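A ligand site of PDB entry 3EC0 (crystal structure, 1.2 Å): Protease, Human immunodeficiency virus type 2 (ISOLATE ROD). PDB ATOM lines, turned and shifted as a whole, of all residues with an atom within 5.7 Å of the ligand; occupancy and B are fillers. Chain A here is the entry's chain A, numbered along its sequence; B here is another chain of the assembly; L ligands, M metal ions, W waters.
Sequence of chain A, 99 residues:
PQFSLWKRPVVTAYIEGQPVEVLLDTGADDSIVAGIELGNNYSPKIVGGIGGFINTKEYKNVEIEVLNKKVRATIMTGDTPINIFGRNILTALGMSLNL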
ATOM      1  N   ARG A   8      18.485 -15.997  17.384  1.00  0.00           N
ATOM      2  CA  ARG A   8      17.246 -16.690  17.743  1.00  0.00           C
ATOM      3  C   ARG A   8      16.269 -16.684  16.572  1.00  0.00           C
ATOM      4  O   ARG A   8      16.066 -15.620  15.976  1.00  0.00           O
ATOM      5  CB  ARG A   8      16.567 -16.045  18.952  1.00  0.00           C
ATOM      6  CG  ARG A   8      17.372 -16.053  20.237  1.00  0.00           C
ATOM      7  CD  ARG A   8      16.580 -15.460  21.375  1.00  0.00           C
ATOM      8  NE  ARG A   8      17.203 -15.616  22.664  1.00  0.00           N
ATOM      9  CZ  ARG A   8      16.779 -15.196  23.839  1.00  0.00           C
ATOM     10  NH1 ARG A   8      15.622 -14.558  23.952  1.00  0.00           N
ATOM     11  NH2 ARG A   8      17.484 -15.435  24.930  1.00  0.00           N
ATOM     12  N   LEU A  23       9.178 -17.507  19.195  1.00  0.00           N
ATOM     13  CA  LEU A  23      10.384 -18.251  19.002  1.00  0.00           C
ATOM     14  C   LEU A  23      10.045 -19.632  18.434  1.00  0.00           C
ATOM     15  O   LEU A  23       9.229 -20.360  19.002  1.00  0.00           O
ATOM     16  CB  LEU A  23      11.009 -18.457  20.380  1.00  0.00           C
ATOM     17  CG  LEU A  23      12.322 -19.207  20.490  1.00  0.00           C
ATOM     18  CD1 LEU A  23      13.439 -18.466  19.757  1.00  0.00           C
ATOM     19  CD2 LEU A  23      12.676 -19.403  21.959  1.00  0.00           C
ATOM     20  N   ASP A  25      10.730 -23.148  18.132  1.00  0.00           N
ATOM     21  CA  ASP A  25      11.455 -23.901  19.133  1.00  0.00           C
ATOM     22  C   ASP A  25      11.315 -25.412  19.014  1.00  0.00           C
ATOM     23  O   ASP A  25      10.344 -26.009  19.449  1.00  0.00           O
ATOM     24  CB  ASP A  25      10.934 -23.495  20.499  1.00  0.00           C
ATOM     25  CG  ASP A  25      11.896 -23.901  21.598  1.00  0.00           C
ATOM     26  OD1 ASP A  25      12.807 -24.721  21.345  1.00  0.00           O
ATOM     27  OD2 ASP A  25      11.709 -23.410  22.739  1.00  0.00           O
ATOM     28  N   GLY A  27      12.845 -27.474  20.746  1.00  0.00           N
ATOM     29  CA  GLY A  27      12.984 -28.067  22.051  1.00  0.00           C
ATOM     30  C   GLY A  27      11.712 -28.011  22.880  1.00  0.00           C
ATOM     31  O   GLY A  27      11.736 -28.387  24.070  1.00  0.00           O
ATOM     32  N   ALA A  28      10.620 -27.592  22.311  1.00  0.00           N
ATOM     33  CA  ALA A  28       9.319 -27.449  22.952  1.00  0.00           C
ATOM     34  C   ALA A  28       8.353 -28.428  22.291  1.00  0.00           C
ATOM     35  O   ALA A  28       8.159 -28.322  21.067  1.00  0.00           O
ATOM     36  CB  ALA A  28       8.833 -26.015  22.812  1.00  0.00           C
ATOM     37  N   ASP A  29       7.714 -29.322  23.023  1.00  0.00           N
ATOM     38  CA  ASP A  29       6.728 -30.168  22.404  1.00  0.00           C
ATOM     39  C   ASP A  29       5.508 -29.383  21.919  1.00  0.00           C
ATOM     40  O   ASP A  29       4.922 -29.683  20.870  1.00  0.00           O
ATOM     41  CB  ASP A  29       6.218 -31.187  23.392  1.00  0.00           C
ATOM     42  CG  ASP A  29       7.188 -32.224  23.883  1.00  0.00           C
ATOM     43  OD1 ASP A  29       8.229 -32.450  23.265  1.00  0.00           O
ATOM     44  OD2 ASP A  29       6.872 -32.832  24.936  1.00  0.00           O
ATOM     45  N   ASP A  30       5.141 -28.406  22.741  1.00  0.00           N
ATOM     46  CA  ASP A  30       3.929 -27.623  22.657  1.00  0.00           C
ATOM     47  C   ASP A  30       4.264 -26.129  22.519  1.00  0.00           C
ATOM     48  O   ASP A  30       5.438 -25.794  22.453  1.00  0.00           O
ATOM     49  CB  ASP A  30       3.063 -27.832  23.904  1.00  0.00           C
ATOM     50  CG  ASP A  30       2.871 -29.294  24.221  1.00  0.00           C
ATOM     51  OD1 ASP A  30       2.109 -29.934  23.476  1.00  0.00           O
ATOM     52  OD2 ASP A  30       3.472 -29.762  25.198  1.00  0.00           O
ATOM     53  N   SER A  31       3.205 -25.344  22.474  1.00  0.00           N
ATOM     54  CA  SER A  31       3.337 -23.889  22.279  1.00  0.00           C
ATOM     55  C   SER A  31       2.708 -23.144  23.434  1.00  0.00           C
ATOM     56  O   SER A  31       1.639 -23.539  23.944  1.00  0.00           O
ATOM     57  CB  SER A  31       2.699 -23.524  20.934  1.00  0.00           C
ATOM     58  OG  SER A  31       3.373 -24.237  19.872  1.00  0.00           O
ATOM     59  N   ILE A  32       3.389 -22.075  23.860  1.00  0.00           N
ATOM     60  CA  ILE A  32       2.976 -21.292  25.007  1.00  0.00           C
ATOM     61  C   ILE A  32       3.229 -19.828  24.724  1.00  0.00           C
ATOM     62  O   ILE A  32       4.320 -19.446  24.314  1.00  0.00           O
ATOM     63  CB  ILE A  32       3.766 -21.729  26.274  1.00  0.00           C
ATOM     64  CG1 ILE A  32       3.796 -23.219  26.550  1.00  0.00           C
ATOM     65  CG2 ILE A  32       3.179 -20.977  27.441  1.00  0.00           C
ATOM     66  CD1 ILE A  32       4.779 -23.674  27.605  1.00  0.00           C
ATOM     67  N   VAL A  47       3.373 -27.035  33.103  1.00  0.00           N
ATOM     68  CA  VAL A  47       4.529 -27.414  32.314  1.00  0.00           C
ATOM     69  C   VAL A  47       5.794 -27.030  33.066  1.00  0.00           C
ATOM     70  O   VAL A  47       5.778 -26.203  33.956  1.00  0.00           O
ATOM     71  CB  VAL A  47       4.563 -26.769  30.931  1.00  0.00           C
ATOM     72  CG1 VAL A  47       3.311 -27.155  30.134  1.00  0.00           C
ATOM     73  CG2 VAL A  47       4.683 -25.265  30.986  1.00  0.00           C
ATOM     74  N   GLY A  48       6.894 -27.658  32.708  1.00  0.00           N
ATOM     75  CA  GLY A  48       8.150 -27.520  33.424  1.00  0.00           C
ATOM     76  C   GLY A  48       9.291 -27.307  32.458  1.00  0.00           C
ATOM     77  O   GLY A  48       9.283 -27.787  31.332  1.00  0.00           O
ATOM     78  N   GLY A  49      10.292 -26.601  32.905  1.00  0.00           N
ATOM     79  CA  GLY A  49      11.546 -26.453  32.200  1.00  0.00           C
ATOM     80  C   GLY A  49      12.635 -25.986  33.145  1.00  0.00           C
ATOM     81  O   GLY A  49      12.591 -26.262  34.351  1.00  0.00           O
ATOM     82  N   ILE A  50      13.607 -25.259  32.559  1.00  0.00           N
ATOM     83  CA  ILE A  50      14.661 -24.701  33.419  1.00  0.00           C
ATOM     84  C   ILE A  50      14.057 -23.626  34.327  1.00  0.00           C
ATOM     85  O   ILE A  50      13.337 -22.720  33.929  1.00  0.00           O
ATOM     86  CB  ILE A  50      15.847 -24.195  32.600  1.00  0.00           C
ATOM     87  CG1 ILE A  50      16.598 -25.372  31.941  1.00  0.00           C
ATOM     88  CG2 ILE A  50      16.844 -23.353  33.390  1.00  0.00           C
ATOM     89  CD1 ILE A  50      17.567 -25.001  30.887  1.00  0.00           C
ATOM     90  N   MET A  76      -1.135 -23.011  24.588  1.00  0.00           N
ATOM     91  CA  MET A  76      -1.243 -22.720  25.994  1.00  0.00           C
ATOM     92  C   MET A  76      -1.008 -21.247  26.249  1.00  0.00           C
ATOM     93  O   MET A  76      -0.128 -20.652  25.601  1.00  0.00           O
ATOM     94  CB  MET A  76      -0.205 -23.548  26.776  1.00  0.00           C
ATOM     95  CG  MET A  76      -0.678 -24.969  27.131  1.00  0.00           C
ATOM     96  SD  MET A  76       0.648 -25.950  27.796  1.00  0.00           S
ATOM     97  CE  MET A  76       1.672 -26.100  26.337  1.00  0.00           C
ATOM     98  N   THR A  80       4.822 -17.217  30.650  1.00  0.00           N
ATOM     99  CA  THR A  80       6.102 -17.555  30.053  1.00  0.00           C
ATOM    100  C   THR A  80       6.885 -16.292  29.732  1.00  0.00           C
ATOM    101  O   THR A  80       6.290 -15.306  29.307  1.00  0.00           O
ATOM    102  CB  THR A  80       5.859 -18.423  28.797  1.00  0.00           C
ATOM    103  OG1 THR A  80       7.140 -18.704  28.265  1.00  0.00           O
ATOM    104  CG2 THR A  80       5.013 -17.712  27.752  1.00  0.00           C
ATOM    105  N   PRO A  81       8.205 -16.295  29.942  1.00  0.00           N
ATOM    106  CA  PRO A  81       8.991 -15.093  29.646  1.00  0.00           C
ATOM    107  C   PRO A  81       9.233 -14.834  28.160  1.00  0.00           C
ATOM    108  O   PRO A  81       9.652 -13.708  27.792  1.00  0.00           O
ATOM    109  CB  PRO A  81      10.334 -15.350  30.345  1.00  0.00           C
ATOM    110  CG  PRO A  81      10.422 -16.843  30.312  1.00  0.00           C
ATOM    111  CD  PRO A  81       9.016 -17.372  30.507  1.00  0.00           C
ATOM    112  N   ILE A  82       8.917 -15.810  27.337  1.00  0.00           N
ATOM    113  CA  ILE A  82       9.077 -15.702  25.884  1.00  0.00           C
ATOM    114  C   ILE A  82       7.958 -16.505  25.262  1.00  0.00           C
ATOM    115  O   ILE A  82       7.498 -17.499  25.828  1.00  0.00           O
ATOM    116  CB  ILE A  82      10.477 -16.141  25.463  1.00  0.00           C
ATOM    117  CG1 ILE A  82      10.836 -15.820  24.008  1.00  0.00           C
ATOM    118  CG2 ILE A  82      10.667 -17.610  25.745  1.00  0.00           C
ATOM    119  CD1 ILE A  82      12.321 -15.806  23.744  1.00  0.00           C
ATOM    120  N   ILE A  84       6.546 -19.099  22.650  1.00  0.00           N
ATOM    121  CA  ILE A  84       7.155 -20.288  22.072  1.00  0.00           C
ATOM    122  C   ILE A  84       6.162 -21.021  21.168  1.00  0.00           C
ATOM    123  O   ILE A  84       5.083 -21.388  21.610  1.00  0.00           O
ATOM    124  CB  ILE A  84       7.622 -21.216  23.198  1.00  0.00           C
ATOM    125  CG1 ILE A  84       8.734 -20.557  24.040  1.00  0.00           C
ATOM    126  CG2 ILE A  84       8.087 -22.555  22.652  1.00  0.00           C
ATOM    127  CD1 ILE A  84       8.951 -21.240  25.371  1.00  0.00           C
ATOM    128  N   LEU B  23      18.528 -33.083  23.569  1.00  0.00           N
ATOM    129  CA  LEU B  23      17.494 -32.494  22.756  1.00  0.00           C
ATOM    130  C   LEU B  23      18.101 -31.373  21.964  1.00  0.00           C
ATOM    131  O   LEU B  23      18.668 -30.437  22.528  1.00  0.00           O
ATOM    132  CB  LEU B  23      16.357 -31.968  23.670  1.00  0.00           C
ATOM    133  CG  LEU B  23      15.159 -31.318  23.086  1.00  0.00           C
ATOM    134  CD1 LEU B  23      14.364 -32.219  22.132  1.00  0.00           C
ATOM    135  CD2 LEU B  23      14.217 -30.839  24.194  1.00  0.00           C
ATOM    136  N   ASP B  25      17.796 -28.116  20.379  1.00  0.00           N
ATOM    137  CA  ASP B  25      16.868 -27.110  20.850  1.00  0.00           C
ATOM    138  C   ASP B  25      17.107 -25.724  20.273  1.00  0.00           C
ATOM    139  O   ASP B  25      17.971 -24.984  20.735  1.00  0.00           O
ATOM    140  CB  ASP B  25      17.068 -27.085  22.381  1.00  0.00           C
ATOM    141  CG  ASP B  25      16.066 -26.298  23.170  1.00  0.00           C
ATOM    142  OD1 ASP B  25      15.289 -25.554  22.519  1.00  0.00           O
ATOM    143  OD2 ASP B  25      15.983 -26.349  24.427  1.00  0.00           O
ATOM    144  N   THR B  26      16.325 -25.408  19.242  1.00  0.00           N
ATOM    145  CA  THR B  26      16.548 -24.107  18.574  1.00  0.00           C
ATOM    146  C   THR B  26      16.099 -22.954  19.448  1.00  0.00           C
ATOM    147  O   THR B  26      16.497 -21.820  19.136  1.00  0.00           O
ATOM    148  CB  THR B  26      15.856 -24.041  17.202  1.00  0.00           C
ATOM    149  OG1 THR B  26      14.455 -24.263  17.408  1.00  0.00           O
ATOM    150  CG2 THR B  26      16.390 -25.078  16.232  1.00  0.00           C
ATOM    151  N   GLY B  27      15.329 -23.235  20.493  1.00  0.00           N
ATOM    152  CA  GLY B  27      14.925 -22.213  21.457  1.00  0.00           C
ATOM    153  C   GLY B  27      15.917 -21.933  22.549  1.00  0.00           C
ATOM    154  O   GLY B  27      15.649 -21.126  23.427  1.00  0.00           O
ATOM    155  N   ALA B  28      17.084 -22.587  22.544  1.00  0.00           N
ATOM    156  CA  ALA B  28      18.106 -22.405  23.569  1.00  0.00           C
ATOM    157  C   ALA B  28      19.305 -21.725  22.956  1.00  0.00           C
ATOM    158  O   ALA B  28      19.794 -22.110  21.881  1.00  0.00           O
ATOM    159  CB  ALA B  28      18.506 -23.762  24.131  1.00  0.00           C
ATOM    160  N   ASP B  29      19.770 -20.676  23.651  1.00  0.00           N
ATOM    161  CA  ASP B  29      20.962 -19.983  23.204  1.00  0.00           C
ATOM    162  C   ASP B  29      22.227 -20.792  23.525  1.00  0.00           C
ATOM    163  O   ASP B  29      23.217 -20.719  22.766  1.00  0.00           O
ATOM    164  CB  ASP B  29      21.123 -18.664  23.913  1.00  0.00           C
ATOM    165  CG  ASP B  29      19.989 -17.667  23.770  1.00  0.00           C
ATOM    166  OD1 ASP B  29      19.190 -17.773  22.791  1.00  0.00           O
ATOM    167  OD2 ASP B  29      19.908 -16.807  24.687  1.00  0.00           O
ATOM    168  N   ASP B  30      22.149 -21.500  24.662  1.00  0.00           N
ATOM    169  CA  ASP B  30      23.292 -22.152  25.292  1.00  0.00           C
ATOM    170  C   ASP B  30      23.002 -23.650  25.356  1.00  0.00           C
ATOM    171  O   ASP B  30      21.854 -24.031  25.118  1.00  0.00           O
ATOM    172  CB  ASP B  30      23.526 -21.656  26.696  1.00  0.00           C
ATOM    173  CG  ASP B  30      23.670 -20.143  26.727  1.00  0.00           C
ATOM    174  OD1 ASP B  30      24.685 -19.637  26.207  1.00  0.00           O
ATOM    175  OD2 ASP B  30      22.814 -19.414  27.227  1.00  0.00           O
ATOM    176  N   ILE B  32      22.962 -26.823  27.934  1.00  0.00           N
ATOM    177  CA  ILE B  32      22.857 -27.053  29.335  1.00  0.00           C
ATOM    178  C   ILE B  32      22.643 -28.543  29.543  1.00  0.00           C
ATOM    179  O   ILE B  32      21.704 -29.109  28.986  1.00  0.00           O
ATOM    180  CB  ILE B  32      21.673 -26.280  29.991  1.00  0.00           C
ATOM    181  CG1 ILE B  32      21.408 -24.863  29.519  1.00  0.00           C
ATOM    182  CG2 ILE B  32      21.783 -26.367  31.528  1.00  0.00           C
ATOM    183  CD1 ILE B  32      22.318 -23.752  29.736  1.00  0.00           C
ATOM    184  N   VAL B  47      21.482 -18.557  34.270  1.00  0.00           N
ATOM    185  CA  VAL B  47      20.673 -18.908  33.107  1.00  0.00           C
ATOM    186  C   VAL B  47      19.192 -18.806  33.454  1.00  0.00           C
ATOM    187  O   VAL B  47      18.805 -19.372  34.481  1.00  0.00           O
ATOM    188  CB  VAL B  47      21.014 -20.349  32.669  1.00  0.00           C
ATOM    189  CG1 VAL B  47      20.045 -20.849  31.650  1.00  0.00           C
ATOM    190  CG2 VAL B  47      22.453 -20.340  32.098  1.00  0.00           C
ATOM    191  N   GLY B  48      18.413 -18.101  32.646  1.00  0.00           N
ATOM    192  CA  GLY B  48      17.006 -17.918  32.774  1.00  0.00           C
ATOM    193  C   GLY B  48      16.153 -18.759  31.841  1.00  0.00           C
ATOM    194  O   GLY B  48      16.205 -18.486  30.657  1.00  0.00           O
ATOM    195  N   GLY B  49      15.423 -19.725  32.382  1.00  0.00           N
ATOM    196  CA  GLY B  49      14.498 -20.568  31.605  1.00  0.00           C
ATOM    197  C   GLY B  49      13.028 -20.243  31.841  1.00  0.00           C
ATOM    198  O   GLY B  49      12.690 -19.176  32.384  1.00  0.00           O
ATOM    199  N   ILE B  50      12.145 -21.123  31.451  1.00  0.00           N
ATOM    200  CA  ILE B  50      10.715 -20.840  31.513  1.00  0.00           C
ATOM    201  C   ILE B  50      10.253 -20.557  32.929  1.00  0.00           C
ATOM    202  O   ILE B  50       9.326 -19.764  33.153  1.00  0.00           O
ATOM    203  CB  ILE B  50       9.864 -21.999  30.941  1.00  0.00           C
ATOM    204  CG1 ILE B  50       8.465 -21.474  30.620  1.00  0.00           C
ATOM    205  CG2 ILE B  50       9.803 -23.228  31.813  1.00  0.00           C
ATOM    206  CD1 ILE B  50       7.730 -22.352  29.621  1.00  0.00           C
ATOM    207  N   THR B  80      18.870 -28.789  34.767  1.00  0.00           N
ATOM    208  CA  THR B  80      17.872 -28.759  33.707  1.00  0.00           C
ATOM    209  C   THR B  80      17.171 -30.104  33.683  1.00  0.00           C
ATOM    210  O   THR B  80      17.852 -31.130  33.851  1.00  0.00           O
ATOM    211  CB  THR B  80      18.525 -28.482  32.341  1.00  0.00           C
ATOM    212  OG1 THR B  80      17.495 -28.529  31.328  1.00  0.00           O
ATOM    213  CG2 THR B  80      19.614 -29.490  31.934  1.00  0.00           C
ATOM    214  N   PRO B  81      15.869 -30.197  33.449  1.00  0.00           N
ATOM    215  CA  PRO B  81      15.169 -31.497  33.425  1.00  0.00           C
ATOM    216  C   PRO B  81      15.442 -32.287  32.158  1.00  0.00           C
ATOM    217  O   PRO B  81      15.168 -33.487  32.162  1.00  0.00           O
ATOM    218  CB  PRO B  81      13.713 -31.072  33.476  1.00  0.00           C
ATOM    219  CG  PRO B  81      13.629 -29.697  32.902  1.00  0.00           C
ATOM    220  CD  PRO B  81      14.960 -29.057  33.251  1.00  0.00           C
ATOM    221  N   ILE B  82      15.931 -31.640  31.134  1.00  0.00           N
ATOM    222  CA  ILE B  82      16.249 -32.260  29.837  1.00  0.00           C
ATOM    223  C   ILE B  82      17.555 -31.654  29.377  1.00  0.00           C
ATOM    224  O   ILE B  82      17.710 -30.421  29.425  1.00  0.00           O
ATOM    225  CB  ILE B  82      15.157 -32.031  28.794  1.00  0.00           C
ATOM    226  CG1 ILE B  82      13.817 -32.614  29.225  1.00  0.00           C
ATOM    227  CG2 ILE B  82      15.599 -32.579  27.443  1.00  0.00           C
ATOM    228  CD1 ILE B  82      12.630 -32.403  28.315  1.00  0.00           C
ATOM    229  N   ILE B  84      19.999 -30.104  26.868  1.00  0.00           N
ATOM    230  CA  ILE B  84      19.731 -29.393  25.634  1.00  0.00           C
ATOM    231  C   ILE B  84      21.003 -28.928  24.959  1.00  0.00           C
ATOM    232  O   ILE B  84      21.927 -28.403  25.594  1.00  0.00           O
ATOM    233  CB  ILE B  84      18.792 -28.200  25.856  1.00  0.00           C
ATOM    234  CG1 ILE B  84      19.321 -27.164  26.841  1.00  0.00           C
ATOM    235  CG2 ILE B  84      17.428 -28.721  26.269  1.00  0.00           C
ATOM    236  CD1 ILE B  84      18.452 -25.967  27.113  1.00  0.00           C
HETATM  237  C1  LIG L   1      17.943 -22.042  28.160  1.00  0.00           C
HETATM  238  C2  LIG L   1      17.538 -20.811  28.980  1.00  0.00           C
HETATM  239  O1  LIG L   1      18.722 -19.838  26.064  1.00  0.00           O
HETATM  240  C3  LIG L   1      17.469 -19.160  26.226  1.00  0.00           C
HETATM  241  C4  LIG L   1      18.319 -19.612  28.397  1.00  0.00           C
HETATM  242  C5  LIG L   1      19.303 -21.699  27.564  1.00  0.00           C
HETATM  243  C6  LIG L   1      17.529 -18.536  27.618  1.00  0.00           C
HETATM  244  C7  LIG L   1      19.309 -20.178  27.321  1.00  0.00           C
HETATM  245  O2  LIG L   1      17.077 -22.207  27.001  1.00  0.00           O
HETATM  246  C8  LIG L   1      15.819 -22.629  27.257  1.00  0.00           C
HETATM  247  C9  LIG L   1      13.636 -22.922  26.164  1.00  0.00           C
HETATM  248  C10 LIG L   1      12.819 -21.754  25.564  1.00  0.00           C
HETATM  249  C11 LIG L   1      13.071 -20.503  26.357  1.00  0.00           C
HETATM  250  C12 LIG L   1      13.826 -19.437  25.815  1.00  0.00           C
HETATM  251  C13 LIG L   1      14.071 -18.270  26.553  1.00  0.00           C
HETATM  252  C14 LIG L   1      13.551 -18.161  27.845  1.00  0.00           C
HETATM  253  C15 LIG L   1      12.791 -19.204  28.410  1.00  0.00           C
HETATM  254  C16 LIG L   1      12.565 -20.384  27.647  1.00  0.00           C
HETATM  255  O3  LIG L   1      15.501 -23.031  28.359  1.00  0.00           O
HETATM  256  N1  LIG L   1      15.067 -22.539  26.138  1.00  0.00           N
HETATM  257  C17 LIG L   1      13.484 -24.260  25.402  1.00  0.00           C
HETATM  258  C18 LIG L   1      12.115 -24.895  25.561  1.00  0.00           C
HETATM  259  C19 LIG L   1      12.097 -26.849  27.197  1.00  0.00           C
HETATM  260  C20 LIG L   1      13.574 -27.257  27.194  1.00  0.00           C
HETATM  261  C21 LIG L   1      14.279 -26.577  28.393  1.00  0.00           C
HETATM  262  C22 LIG L   1      13.570 -28.811  27.431  1.00  0.00           C
HETATM  263  O4  LIG L   1      13.762 -24.082  24.006  1.00  0.00           O
HETATM  264  O5  LIG L   1      10.712 -23.301  27.408  1.00  0.00           O
HETATM  265  O6  LIG L   1      11.091 -24.909  29.227  1.00  0.00           O
HETATM  266  N2  LIG L   1      11.910 -25.404  26.937  1.00  0.00           N
HETATM  267  S1  LIG L   1      10.774 -24.670  27.855  1.00  0.00           S
HETATM  268  C23 LIG L   1       9.184 -25.414  27.587  1.00  0.00           C
HETATM  269  C24 LIG L   1       8.456 -24.992  26.448  1.00  0.00           C
HETATM  270  C25 LIG L   1       7.273 -25.644  26.166  1.00  0.00           C
HETATM  271  C26 LIG L   1       6.825 -26.659  26.997  1.00  0.00           C
HETATM  272  C27 LIG L   1       7.562 -27.055  28.105  1.00  0.00           C
HETATM  273  C28 LIG L   1       8.787 -26.429  28.438  1.00  0.00           C
HETATM  274  C29 LIG L   1       5.514 -27.308  26.613  1.00  0.00           C
HETATM  275  O7  LIG L   1       5.765 -28.417  25.781  1.00  0.00           O
HETATM  276 ZN    ZN M   1      22.512 -17.764  28.111  1.00  0.00          ZN
HETATM  277 ZN    ZN M   2      23.175 -17.521  26.969  1.00  0.00          ZN
HETATM  278  O   HOH W   1      13.328 -23.507  30.149  1.00  0.00           O
HETATM  279  O   HOH W   2       8.200 -29.810  25.803  1.00  0.00           O
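The side-chain carboxylate (OD1) of Asp 25 of chain A is in hydrogen-bond range of the backbone NH (N) of Gly 27 of chain B, 3.0 Å away. The side-chain carboxylate (OD1) of Asp 25 of chain A sits at hydrogen-bond distance from the backbone NH (N) of Gly 27 of chain A (2.8 Å). N of Gly 27 of chain B sits close to OD1 of Asp 25 of chain B (3.1 Å). N of Ala 28 of chain B sits at hydrogen-bond distance from OD1 of Asp 25 of chain B, 3.5 Å away. The side-chain carboxylate (OD2) of Asp 29 of chain B is in salt-bridge range of the guanidinium group (NH2) of Arg 8 (2.8 Å). The backbone NH (N) of Ile 50 of chain B sits at hydrogen-bond distance from the backbone carbonyl oxygen (O) of Ile 50 of chain A. The backbone NH (N) of Ile 84 of chain A sits at hydrogen-bond distance from the backbone carbonyl oxygen (O) of Ile 32 of chain A, at 2.8 Å. OG1 of Thr 80 of chain B lies within hydrogen-bond range of O of Ile 82 of chain B, at 2.7 Å.
Water W1 lies within hydrogen-bond range of O6 of the ligand (2.8 Å), N of Ile 50 of chain B (3.0 Å) and N of Ile 50 of chain A (3.0 Å). Water W2 lies within hydrogen-bond range of an oxygen (O7) of the ligand and the backbone NH of Asp 29 of chain A.
O4 of the ligand lies within hydrogen-bond range of OD2 of Asp 25 of chain A (2.5 Å). OD1 of Asp 25 of chain B sits at hydrogen-bond distance from O4 of the ligand (2.6 Å). An oxygen (O7) of the ligand sits at hydrogen-bond distance from the backbone NH (N) of Asp 30 of chain A, 3.1 Å away. O7 of the ligand sits at hydrogen-bond distance from OD2 of Asp 30 of chain A. An oxygen (O1) of the ligand lies within hydrogen-bond range of the backbone NH (N) of Asp 29 of chain B. A nitrogen (N1) of the ligand is in hydrogen-bond range of the backbone carbonyl oxygen (O) of Gly 27 of chain B (3.1 Å). The backbone NH of Asp 29 of chain A lies within hydrogen-bond range of an oxygen (O7) of the ligand.
Residues that only touch the ligand: Gly 48 of chain B, Gly 48 of chain A, Ile 50 of chain B, Gly 49 of chain A, Ile 84 of chain A, Ile 32 of chain A, Gly 27 of chain A, Ile 82 of chain A, Ala 28 of chain B, Asp 30 of chain B, Gly 49 of chain B, Val 47 of chain B, Ala 28 of chain A, Ile 50 of chain A, Ile 82 of chain B, Pro 81 of chain A, Leu 23 of chain B and Arg 8. Hydrophobic or aromatic side chains that line the ligand: Ala 28 of chain A, Ile 32 of chain A, Ile 50 of chain A, Pro 81 of chain A, Ile 82 of chain A, Ile 84 of chain A, Leu 23 of chain B, Ala 28 of chain B, Val 47 of chain B, Ile 50 of chain B and Ile 82 of chain B. 24 residues have an atom within 4 Å of the ligand: Arg 8, Asp 25 of chain A, Gly 27 of chain A, Ala 28 of chain A, Asp 29 of chain A, Asp 30 of chain A, Ile 32 of chain A, Gly 48 of chain A, Gly 49 of chain A, Ile 50 of chain A, Pro 81 of chain A, Ile 82 of chain A, Ile 84 of chain A, Leu 23 of chain B, Asp 25 of chain B, Gly 27 of chain B, Ala 28 of chain B, Asp 29 of chain B, Asp 30 of chain B, Val 47 of chain B, Gly 48 of chain B, Gly 49 of chain B, Ile 50 of chain B and Ile 82 of chain B. Along chain A the residues within 4 Å of the ligand span positions 8 to 84. The nearest printed residue that does not touch the ligand is Ile 84 of chain B (4.01 Å).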
